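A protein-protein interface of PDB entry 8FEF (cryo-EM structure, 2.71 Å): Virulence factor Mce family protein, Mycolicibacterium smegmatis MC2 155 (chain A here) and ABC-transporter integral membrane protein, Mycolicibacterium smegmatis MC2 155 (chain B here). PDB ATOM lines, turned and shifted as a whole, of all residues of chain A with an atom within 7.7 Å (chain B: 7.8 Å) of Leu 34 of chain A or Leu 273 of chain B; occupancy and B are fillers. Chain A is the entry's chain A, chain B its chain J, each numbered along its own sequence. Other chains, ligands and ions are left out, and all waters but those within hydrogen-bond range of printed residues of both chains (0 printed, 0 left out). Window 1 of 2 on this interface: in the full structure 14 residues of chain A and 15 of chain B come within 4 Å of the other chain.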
ATOM      1  N   LEU A  28     -36.986  11.188 -19.479  1.00  0.00           N
ATOM      2  CA  LEU A  28     -35.930  10.304 -19.959  1.00  0.00           C
ATOM      3  C   LEU A  28     -34.740  11.102 -20.475  1.00  0.00           C
ATOM      4  O   LEU A  28     -33.586  10.725 -20.245  1.00  0.00           O
ATOM      5  CB  LEU A  28     -36.474   9.381 -21.049  1.00  0.00           C
ATOM      6  CG  LEU A  28     -35.534   8.283 -21.546  1.00  0.00           C
ATOM      7  CD1 LEU A  28     -35.231   7.294 -20.432  1.00  0.00           C
ATOM      8  CD2 LEU A  28     -36.129   7.574 -22.751  1.00  0.00           C
ATOM      9  N   VAL A  29     -35.001  12.212 -21.173  1.00  0.00           N
ATOM     10  CA  VAL A  29     -33.918  13.065 -21.658  1.00  0.00           C
ATOM     11  C   VAL A  29     -33.128  13.644 -20.491  1.00  0.00           C
ATOM     12  O   VAL A  29     -31.891  13.649 -20.503  1.00  0.00           O
ATOM     13  CB  VAL A  29     -34.479  14.171 -22.574  1.00  0.00           C
ATOM     14  CG1 VAL A  29     -33.465  15.292 -22.753  1.00  0.00           C
ATOM     15  CG2 VAL A  29     -34.861  13.591 -23.927  1.00  0.00           C
ATOM     16  N   GLY A  30     -33.828  14.134 -19.465  1.00  0.00           N
ATOM     17  CA  GLY A  30     -33.139  14.663 -18.296  1.00  0.00           C
ATOM     18  C   GLY A  30     -32.295  13.620 -17.588  1.00  0.00           C
ATOM     19  O   GLY A  30     -31.145  13.882 -17.214  1.00  0.00           O
ATOM     20  N   VAL A  31     -32.851  12.420 -17.397  1.00  0.00           N
ATOM     21  CA  VAL A  31     -32.116  11.352 -16.725  1.00  0.00           C
ATOM     22  C   VAL A  31     -30.900  10.941 -17.545  1.00  0.00           C
ATOM     23  O   VAL A  31     -29.815  10.709 -16.997  1.00  0.00           O
ATOM     24  CB  VAL A  31     -33.047  10.158 -16.439  1.00  0.00           C
ATOM     25  CG1 VAL A  31     -32.252   8.958 -15.950  1.00  0.00           C
ATOM     26  CG2 VAL A  31     -34.091  10.546 -15.404  1.00  0.00           C
ATOM     27  N   LEU A  32     -31.056  10.844 -18.869  1.00  0.00           N
ATOM     28  CA  LEU A  32     -29.929  10.479 -19.721  1.00  0.00           C
ATOM     29  C   LEU A  32     -28.841  11.545 -19.696  1.00  0.00           C
ATOM     30  O   LEU A  32     -27.650  11.217 -19.688  1.00  0.00           O
ATOM     31  CB  LEU A  32     -30.405  10.235 -21.152  1.00  0.00           C
ATOM     32  CG  LEU A  32     -30.558   8.775 -21.582  1.00  0.00           C
ATOM     33  CD1 LEU A  32     -31.565   8.048 -20.705  1.00  0.00           C
ATOM     34  CD2 LEU A  32     -30.956   8.687 -23.048  1.00  0.00           C
ATOM     35  N   VAL A  33     -29.226  12.825 -19.688  1.00  0.00           N
ATOM     36  CA  VAL A  33     -28.236  13.896 -19.604  1.00  0.00           C
ATOM     37  C   VAL A  33     -27.475  13.821 -18.286  1.00  0.00           C
ATOM     38  O   VAL A  33     -26.242  13.937 -18.257  1.00  0.00           O
ATOM     39  CB  VAL A  33     -28.910  15.268 -19.796  1.00  0.00           C
ATOM     40  CG1 VAL A  33     -27.975  16.390 -19.374  1.00  0.00           C
ATOM     41  CG2 VAL A  33     -29.321  15.451 -21.248  1.00  0.00           C
ATOM     42  N   LEU A  34     -28.194  13.611 -17.178  1.00  0.00           N
ATOM     43  CA  LEU A  34     -27.530  13.492 -15.880  1.00  0.00           C
ATOM     44  C   LEU A  34     -26.591  12.290 -15.842  1.00  0.00           C
ATOM     45  O   LEU A  34     -25.465  12.387 -15.336  1.00  0.00           O
ATOM     46  CB  LEU A  34     -28.568  13.398 -14.762  1.00  0.00           C
ATOM     47  CG  LEU A  34     -28.939  14.688 -14.023  1.00  0.00           C
ATOM     48  CD1 LEU A  34     -29.505  15.737 -14.969  1.00  0.00           C
ATOM     49  CD2 LEU A  34     -29.919  14.393 -12.899  1.00  0.00           C
ATOM     50  N   ALA A  35     -27.034  11.152 -16.383  1.00  0.00           N
ATOM     51  CA  ALA A  35     -26.206   9.950 -16.376  1.00  0.00           C
ATOM     52  C   ALA A  35     -24.965  10.124 -17.241  1.00  0.00           C
ATOM     53  O   ALA A  35     -23.873   9.693 -16.859  1.00  0.00           O
ATOM     54  CB  ALA A  35     -27.022   8.747 -16.842  1.00  0.00           C
ATOM     55  N   LEU A  36     -25.113  10.744 -18.415  1.00  0.00           N
ATOM     56  CA  LEU A  36     -23.964  10.986 -19.282  1.00  0.00           C
ATOM     57  C   LEU A  36     -22.980  11.956 -18.640  1.00  0.00           C
ATOM     58  O   LEU A  36     -21.763  11.772 -18.751  1.00  0.00           O
ATOM     59  CB  LEU A  36     -24.428  11.508 -20.641  1.00  0.00           C
ATOM     60  CG  LEU A  36     -24.593  10.487 -21.771  1.00  0.00           C
ATOM     61  CD1 LEU A  36     -25.542   9.361 -21.386  1.00  0.00           C
ATOM     62  CD2 LEU A  36     -25.066  11.176 -23.042  1.00  0.00           C
ATOM     63  N   THR A  37     -23.487  12.997 -17.972  1.00  0.00           N
ATOM     64  CA  THR A  37     -22.607  13.909 -17.248  1.00  0.00           C
ATOM     65  C   THR A  37     -21.853  13.191 -16.133  1.00  0.00           C
ATOM     66  O   THR A  37     -20.653  13.419 -15.940  1.00  0.00           O
ATOM     67  CB  THR A  37     -23.413  15.077 -16.682  1.00  0.00           C
ATOM     68  OG1 THR A  37     -24.080  15.762 -17.750  1.00  0.00           O
ATOM     69  CG2 THR A  37     -22.505  16.052 -15.955  1.00  0.00           C
ATOM     70  N   TRP A  38     -22.536  12.311 -15.396  1.00  0.00           N
ATOM     71  CA  TRP A  38     -21.859  11.558 -14.342  1.00  0.00           C
ATOM     72  C   TRP A  38     -20.814  10.603 -14.912  1.00  0.00           C
ATOM     73  O   TRP A  38     -19.728  10.454 -14.339  1.00  0.00           O
ATOM     74  CB  TRP A  38     -22.876  10.794 -13.497  1.00  0.00           C
ATOM     75  CG  TRP A  38     -22.250  10.060 -12.354  1.00  0.00           C
ATOM     76  CD1 TRP A  38     -22.128   8.708 -12.216  1.00  0.00           C
ATOM     77  CD2 TRP A  38     -21.639  10.638 -11.194  1.00  0.00           C
ATOM     78  NE1 TRP A  38     -21.489   8.408 -11.037  1.00  0.00           N
ATOM     79  CE2 TRP A  38     -21.178   9.576 -10.392  1.00  0.00           C
ATOM     80  CE3 TRP A  38     -21.442  11.950 -10.754  1.00  0.00           C
ATOM     81  CZ2 TRP A  38     -20.532   9.786  -9.177  1.00  0.00           C
ATOM     82  CZ3 TRP A  38     -20.802  12.157  -9.547  1.00  0.00           C
ATOM     83  CH2 TRP A  38     -20.354  11.080  -8.772  1.00  0.00           C
ATOM     84  N   MET A  39     -21.127   9.936 -16.026  1.00  0.00           N
ATOM     85  CA  MET A  39     -20.163   9.029 -16.646  1.00  0.00           C
ATOM     86  C   MET A  39     -18.944   9.781 -17.167  1.00  0.00           C
ATOM     87  O   MET A  39     -17.810   9.310 -17.021  1.00  0.00           O
ATOM     88  CB  MET A  39     -20.828   8.238 -17.772  1.00  0.00           C
ATOM     89  CG  MET A  39     -21.861   7.231 -17.298  1.00  0.00           C
ATOM     90  SD  MET A  39     -22.620   6.328 -18.660  1.00  0.00           S
ATOM     91  CE  MET A  39     -21.187   5.524 -19.370  1.00  0.00           C
ATOM     92  N   GLN A  40     -19.158  10.945 -17.785  1.00  0.00           N
ATOM     93  CA  GLN A  40     -18.036  11.758 -18.242  1.00  0.00           C
ATOM     94  C   GLN A  40     -17.228  12.302 -17.070  1.00  0.00           C
ATOM     95  O   GLN A  40     -16.011  12.486 -17.190  1.00  0.00           O
ATOM     96  CB  GLN A  40     -18.549  12.897 -19.126  1.00  0.00           C
ATOM     97  CG  GLN A  40     -17.470  13.800 -19.701  1.00  0.00           C
ATOM     98  CD  GLN A  40     -16.562  13.091 -20.685  1.00  0.00           C
ATOM     99  OE1 GLN A  40     -16.933  12.075 -21.271  1.00  0.00           O
ATOM    100  NE2 GLN A  40     -15.362  13.626 -20.872  1.00  0.00           N
ATOM    101  N   PHE A  41     -17.883  12.562 -15.937  1.00  0.00           N
ATOM    102  CA  PHE A  41     -17.166  13.007 -14.746  1.00  0.00           C
ATOM    103  C   PHE A  41     -16.223  11.926 -14.230  1.00  0.00           C
ATOM    104  O   PHE A  41     -15.104  12.223 -13.795  1.00  0.00           O
ATOM    105  CB  PHE A  41     -18.167  13.416 -13.664  1.00  0.00           C
ATOM    106  CG  PHE A  41     -17.534  13.750 -12.344  1.00  0.00           C
ATOM    107  CD1 PHE A  41     -16.911  14.970 -12.150  1.00  0.00           C
ATOM    108  CD2 PHE A  41     -17.575  12.850 -11.294  1.00  0.00           C
ATOM    109  CE1 PHE A  41     -16.330  15.280 -10.938  1.00  0.00           C
ATOM    110  CE2 PHE A  41     -16.997  13.155 -10.081  1.00  0.00           C
ATOM    111  CZ  PHE A  41     -16.374  14.372  -9.902  1.00  0.00           C
ATOM    112  N   GLU B 226     -21.869  26.929 -22.739  1.00  0.00           N
ATOM    113  CA  GLU B 226     -22.731  26.843 -21.562  1.00  0.00           C
ATOM    114  C   GLU B 226     -23.723  27.994 -21.525  1.00  0.00           C
ATOM    115  O   GLU B 226     -24.911  27.793 -21.248  1.00  0.00           O
ATOM    116  CB  GLU B 226     -21.898  26.854 -20.281  1.00  0.00           C
ATOM    117  CG  GLU B 226     -20.883  25.748 -20.162  1.00  0.00           C
ATOM    118  CD  GLU B 226     -19.971  25.929 -18.965  1.00  0.00           C
ATOM    119  OE1 GLU B 226     -20.127  26.937 -18.245  1.00  0.00           O
ATOM    120  OE2 GLU B 226     -19.098  25.065 -18.744  1.00  0.00           O
ATOM    121  N   ALA B 266     -32.447  26.697 -12.855  1.00  0.00           N
ATOM    122  CA  ALA B 266     -31.979  26.096 -14.099  1.00  0.00           C
ATOM    123  C   ALA B 266     -30.581  26.575 -14.468  1.00  0.00           C
ATOM    124  O   ALA B 266     -29.747  25.779 -14.917  1.00  0.00           O
ATOM    125  CB  ALA B 266     -32.963  26.399 -15.228  1.00  0.00           C
ATOM    126  N   ILE B 267     -30.306  27.872 -14.296  1.00  0.00           N
ATOM    127  CA  ILE B 267     -28.990  28.411 -14.633  1.00  0.00           C
ATOM    128  C   ILE B 267     -27.911  27.761 -13.781  1.00  0.00           C
ATOM    129  O   ILE B 267     -26.872  27.308 -14.292  1.00  0.00           O
ATOM    130  CB  ILE B 267     -28.980  29.940 -14.470  1.00  0.00           C
ATOM    131  CG1 ILE B 267     -29.832  30.592 -15.550  1.00  0.00           C
ATOM    132  CG2 ILE B 267     -27.559  30.479 -14.502  1.00  0.00           C
ATOM    133  CD1 ILE B 267     -30.302  31.965 -15.191  1.00  0.00           C
ATOM    134  N   VAL B 268     -28.138  27.709 -12.463  1.00  0.00           N
ATOM    135  CA  VAL B 268     -27.120  27.133 -11.586  1.00  0.00           C
ATOM    136  C   VAL B 268     -26.900  25.662 -11.921  1.00  0.00           C
ATOM    137  O   VAL B 268     -25.756  25.186 -11.977  1.00  0.00           O
ATOM    138  CB  VAL B 268     -27.498  27.343 -10.109  1.00  0.00           C
ATOM    139  CG1 VAL B 268     -26.443  26.741  -9.211  1.00  0.00           C
ATOM    140  CG2 VAL B 268     -27.643  28.823  -9.815  1.00  0.00           C
ATOM    141  N   LEU B 269     -27.989  24.924 -12.173  1.00  0.00           N
ATOM    142  CA  LEU B 269     -27.863  23.507 -12.499  1.00  0.00           C
ATOM    143  C   LEU B 269     -27.092  23.296 -13.797  1.00  0.00           C
ATOM    144  O   LEU B 269     -26.247  22.395 -13.884  1.00  0.00           O
ATOM    145  CB  LEU B 269     -29.248  22.870 -12.588  1.00  0.00           C
ATOM    146  CG  LEU B 269     -29.331  21.389 -12.231  1.00  0.00           C
ATOM    147  CD1 LEU B 269     -28.859  21.170 -10.807  1.00  0.00           C
ATOM    148  CD2 LEU B 269     -30.748  20.878 -12.414  1.00  0.00           C
ATOM    149  N   VAL B 270     -27.371  24.112 -14.817  1.00  0.00           N
ATOM    150  CA  VAL B 270     -26.692  23.970 -16.104  1.00  0.00           C
ATOM    151  C   VAL B 270     -25.196  24.208 -15.946  1.00  0.00           C
ATOM    152  O   VAL B 270     -24.369  23.436 -16.454  1.00  0.00           O
ATOM    153  CB  VAL B 270     -27.308  24.923 -17.145  1.00  0.00           C
ATOM    154  CG1 VAL B 270     -26.374  25.101 -18.330  1.00  0.00           C
ATOM    155  CG2 VAL B 270     -28.649  24.392 -17.616  1.00  0.00           C
ATOM    156  N   VAL B 271     -24.825  25.280 -15.236  1.00  0.00           N
ATOM    157  CA  VAL B 271     -23.404  25.578 -15.058  1.00  0.00           C
ATOM    158  C   VAL B 271     -22.714  24.454 -14.292  1.00  0.00           C
ATOM    159  O   VAL B 271     -21.607  24.027 -14.654  1.00  0.00           O
ATOM    160  CB  VAL B 271     -23.215  26.940 -14.366  1.00  0.00           C
ATOM    161  CG1 VAL B 271     -21.739  27.233 -14.177  1.00  0.00           C
ATOM    162  CG2 VAL B 271     -23.852  28.034 -15.187  1.00  0.00           C
ATOM    163  N   LEU B 272     -23.355  23.951 -13.230  1.00  0.00           N
ATOM    164  CA  LEU B 272     -22.755  22.872 -12.449  1.00  0.00           C
ATOM    165  C   LEU B 272     -22.542  21.625 -13.297  1.00  0.00           C
ATOM    166  O   LEU B 272     -21.463  21.020 -13.266  1.00  0.00           O
ATOM    167  CB  LEU B 272     -23.627  22.539 -11.239  1.00  0.00           C
ATOM    168  CG  LEU B 272     -23.228  21.239 -10.532  1.00  0.00           C
ATOM    169  CD1 LEU B 272     -21.858  21.365  -9.888  1.00  0.00           C
ATOM    170  CD2 LEU B 272     -24.266  20.800  -9.517  1.00  0.00           C
ATOM    171  N   LEU B 273     -23.563  21.220 -14.058  1.00  0.00           N
ATOM    172  CA  LEU B 273     -23.445  20.007 -14.863  1.00  0.00           C
ATOM    173  C   LEU B 273     -22.365  20.149 -15.925  1.00  0.00           C
ATOM    174  O   LEU B 273     -21.578  19.220 -16.150  1.00  0.00           O
ATOM    175  CB  LEU B 273     -24.786  19.667 -15.511  1.00  0.00           C
ATOM    176  CG  LEU B 273     -25.901  19.189 -14.583  1.00  0.00           C
ATOM    177  CD1 LEU B 273     -27.139  18.827 -15.386  1.00  0.00           C
ATOM    178  CD2 LEU B 273     -25.435  18.010 -13.748  1.00  0.00           C
ATOM    179  N   ALA B 274     -22.310  21.306 -16.590  1.00  0.00           N
ATOM    180  CA  ALA B 274     -21.304  21.507 -17.626  1.00  0.00           C
ATOM    181  C   ALA B 274     -19.893  21.486 -17.052  1.00  0.00           C
ATOM    182  O   ALA B 274     -18.989  20.869 -17.631  1.00  0.00           O
ATOM    183  CB  ALA B 274     -21.569  22.817 -18.358  1.00  0.00           C
ATOM    184  N   SER B 275     -19.681  22.146 -15.908  1.00  0.00           N
ATOM    185  CA  SER B 275     -18.354  22.137 -15.298  1.00  0.00           C
ATOM    186  C   SER B 275     -17.974  20.745 -14.806  1.00  0.00           C
ATOM    187  O   SER B 275     -16.801  20.362 -14.867  1.00  0.00           O
ATOM    188  CB  SER B 275     -18.289  23.146 -14.156  1.00  0.00           C
ATOM    189  OG  SER B 275     -18.236  24.473 -14.650  1.00  0.00           O
ATOM    190  N   LEU B 276     -18.944  19.981 -14.300  1.00  0.00           N
ATOM    191  CA  LEU B 276     -18.656  18.616 -13.873  1.00  0.00           C
ATOM    192  C   LEU B 276     -18.277  17.736 -15.056  1.00  0.00           C
ATOM    193  O   LEU B 276     -17.378  16.893 -14.948  1.00  0.00           O
ATOM    194  CB  LEU B 276     -19.860  18.031 -13.135  1.00  0.00           C
ATOM    195  CG  LEU B 276     -19.645  17.674 -11.665  1.00  0.00           C
ATOM    196  CD1 LEU B 276     -19.123  18.873 -10.898  1.00  0.00           C
ATOM    197  CD2 LEU B 276     -20.936  17.166 -11.049  1.00  0.00           C
ATOM    198  N   ALA B 277     -18.956  17.911 -16.191  1.00  0.00           N
ATOM    199  CA  ALA B 277     -18.656  17.092 -17.361  1.00  0.00           C
ATOM    200  C   ALA B 277     -17.309  17.460 -17.974  1.00  0.00           C
ATOM    201  O   ALA B 277     -16.547  16.575 -18.377  1.00  0.00           O
ATOM    202  CB  ALA B 277     -19.770  17.230 -18.397  1.00  0.00           C
ATOM    203  N   LEU B 278     -16.998  18.756 -18.054  1.00  0.00           N
ATOM    204  CA  LEU B 278     -15.795  19.183 -18.766  1.00  0.00           C
ATOM    205  C   LEU B 278     -14.524  18.802 -18.016  1.00  0.00           C
ATOM    206  O   LEU B 278     -13.588  18.250 -18.605  1.00  0.00           O
ATOM    207  CB  LEU B 278     -15.839  20.689 -19.006  1.00  0.00           C
ATOM    208  CG  LEU B 278     -16.832  21.170 -20.061  1.00  0.00           C
ATOM    209  CD1 LEU B 278     -17.009  22.667 -19.949  1.00  0.00           C
ATOM    210  CD2 LEU B 278     -16.354  20.785 -21.447  1.00  0.00           C
ATOM    211  N   TYR B 279     -14.465  19.091 -16.717  1.00  0.00           N
ATOM    212  CA  TYR B 279     -13.228  18.984 -15.953  1.00  0.00           C
ATOM    213  C   TYR B 279     -13.257  17.841 -14.946  1.00  0.00           C
ATOM    214  O   TYR B 279     -12.505  17.865 -13.968  1.00  0.00           O
ATOM    215  CB  TYR B 279     -12.929  20.303 -15.241  1.00  0.00           C
ATOM    216  CG  TYR B 279     -13.084  21.516 -16.126  1.00  0.00           C
ATOM    217  CD1 TYR B 279     -12.089  21.876 -17.022  1.00  0.00           C
ATOM    218  CD2 TYR B 279     -14.225  22.302 -16.064  1.00  0.00           C
ATOM    219  CE1 TYR B 279     -12.227  22.982 -17.834  1.00  0.00           C
ATOM    220  CE2 TYR B 279     -14.371  23.411 -16.870  1.00  0.00           C
ATOM    221  CZ  TYR B 279     -13.368  23.747 -17.753  1.00  0.00           C
ATOM    222  OH  TYR B 279     -13.510  24.851 -18.560  1.00  0.00           O
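The side-chain hydroxyl (OG1) of Thr 37 of chain A sits at hydrogen-bond distance from the backbone carbonyl oxygen (O) of Val 33 of chain A (2.9 Å).
Among the printed residues, pairs that only touch across the chains: Leu 34 of chain A with Leu 273 of chain B, Thr 37 of chain A with Leu 273 of chain B, Thr 37 of chain A with Ala 277 of chain B, Gln 40 of chain A with Ala 277 of chain B and Phe 41 of chain A with Leu 276 of chain B.
Printed residues of chain A that touch a printed residue of chain B: Leu 34, Thr 37, Gln 40 and Phe 41.
Hydrophobic or aromatic side chains of chain A within 4 Å of the printed part of chain B: Leu 34 and Phe 41.
Along chain A the printed residues that touch a printed residue of chain B span positions 34 to 41.
Among the printed residues, 5 pairs touch across the chains.
Among the printed residues, no Asp or Glu carboxylate lies within 4 Å of a Lys or Arg side-chain nitrogen of the other chain.
Printed residues of chain B within 4 Å of Leu 34 of chain A: Leu 273.
Of the printed residues of chain B, Thr 37 of chain A touches Leu 273 (3.3 Å) and Ala 277 (3.9 Å).
Met 39 of chain A touches none of the printed residues of chain B.
Printed residues of chain B within 4 Å of Gln 40 of chain A: Ala 277 (3.2 Å).
Of chain A, only Leu 34 and Thr 37 come within 4 Å of Leu 273 of chain B.
Of the printed residues of chain A, Leu 276 of chain B touches Phe 41.
The nearest residue of chain B that does not touch Leu 34 of chain A is Leu 269 of chain B (5.9 Å).
The nearest residue of chain A that does not touch Leu 273 of chain B is Val 33 of chain A (4.7 Å).
The nearest printed residue of chain A that does not touch Ala 277 of chain B is Phe 41 of chain A (4.8 Å).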
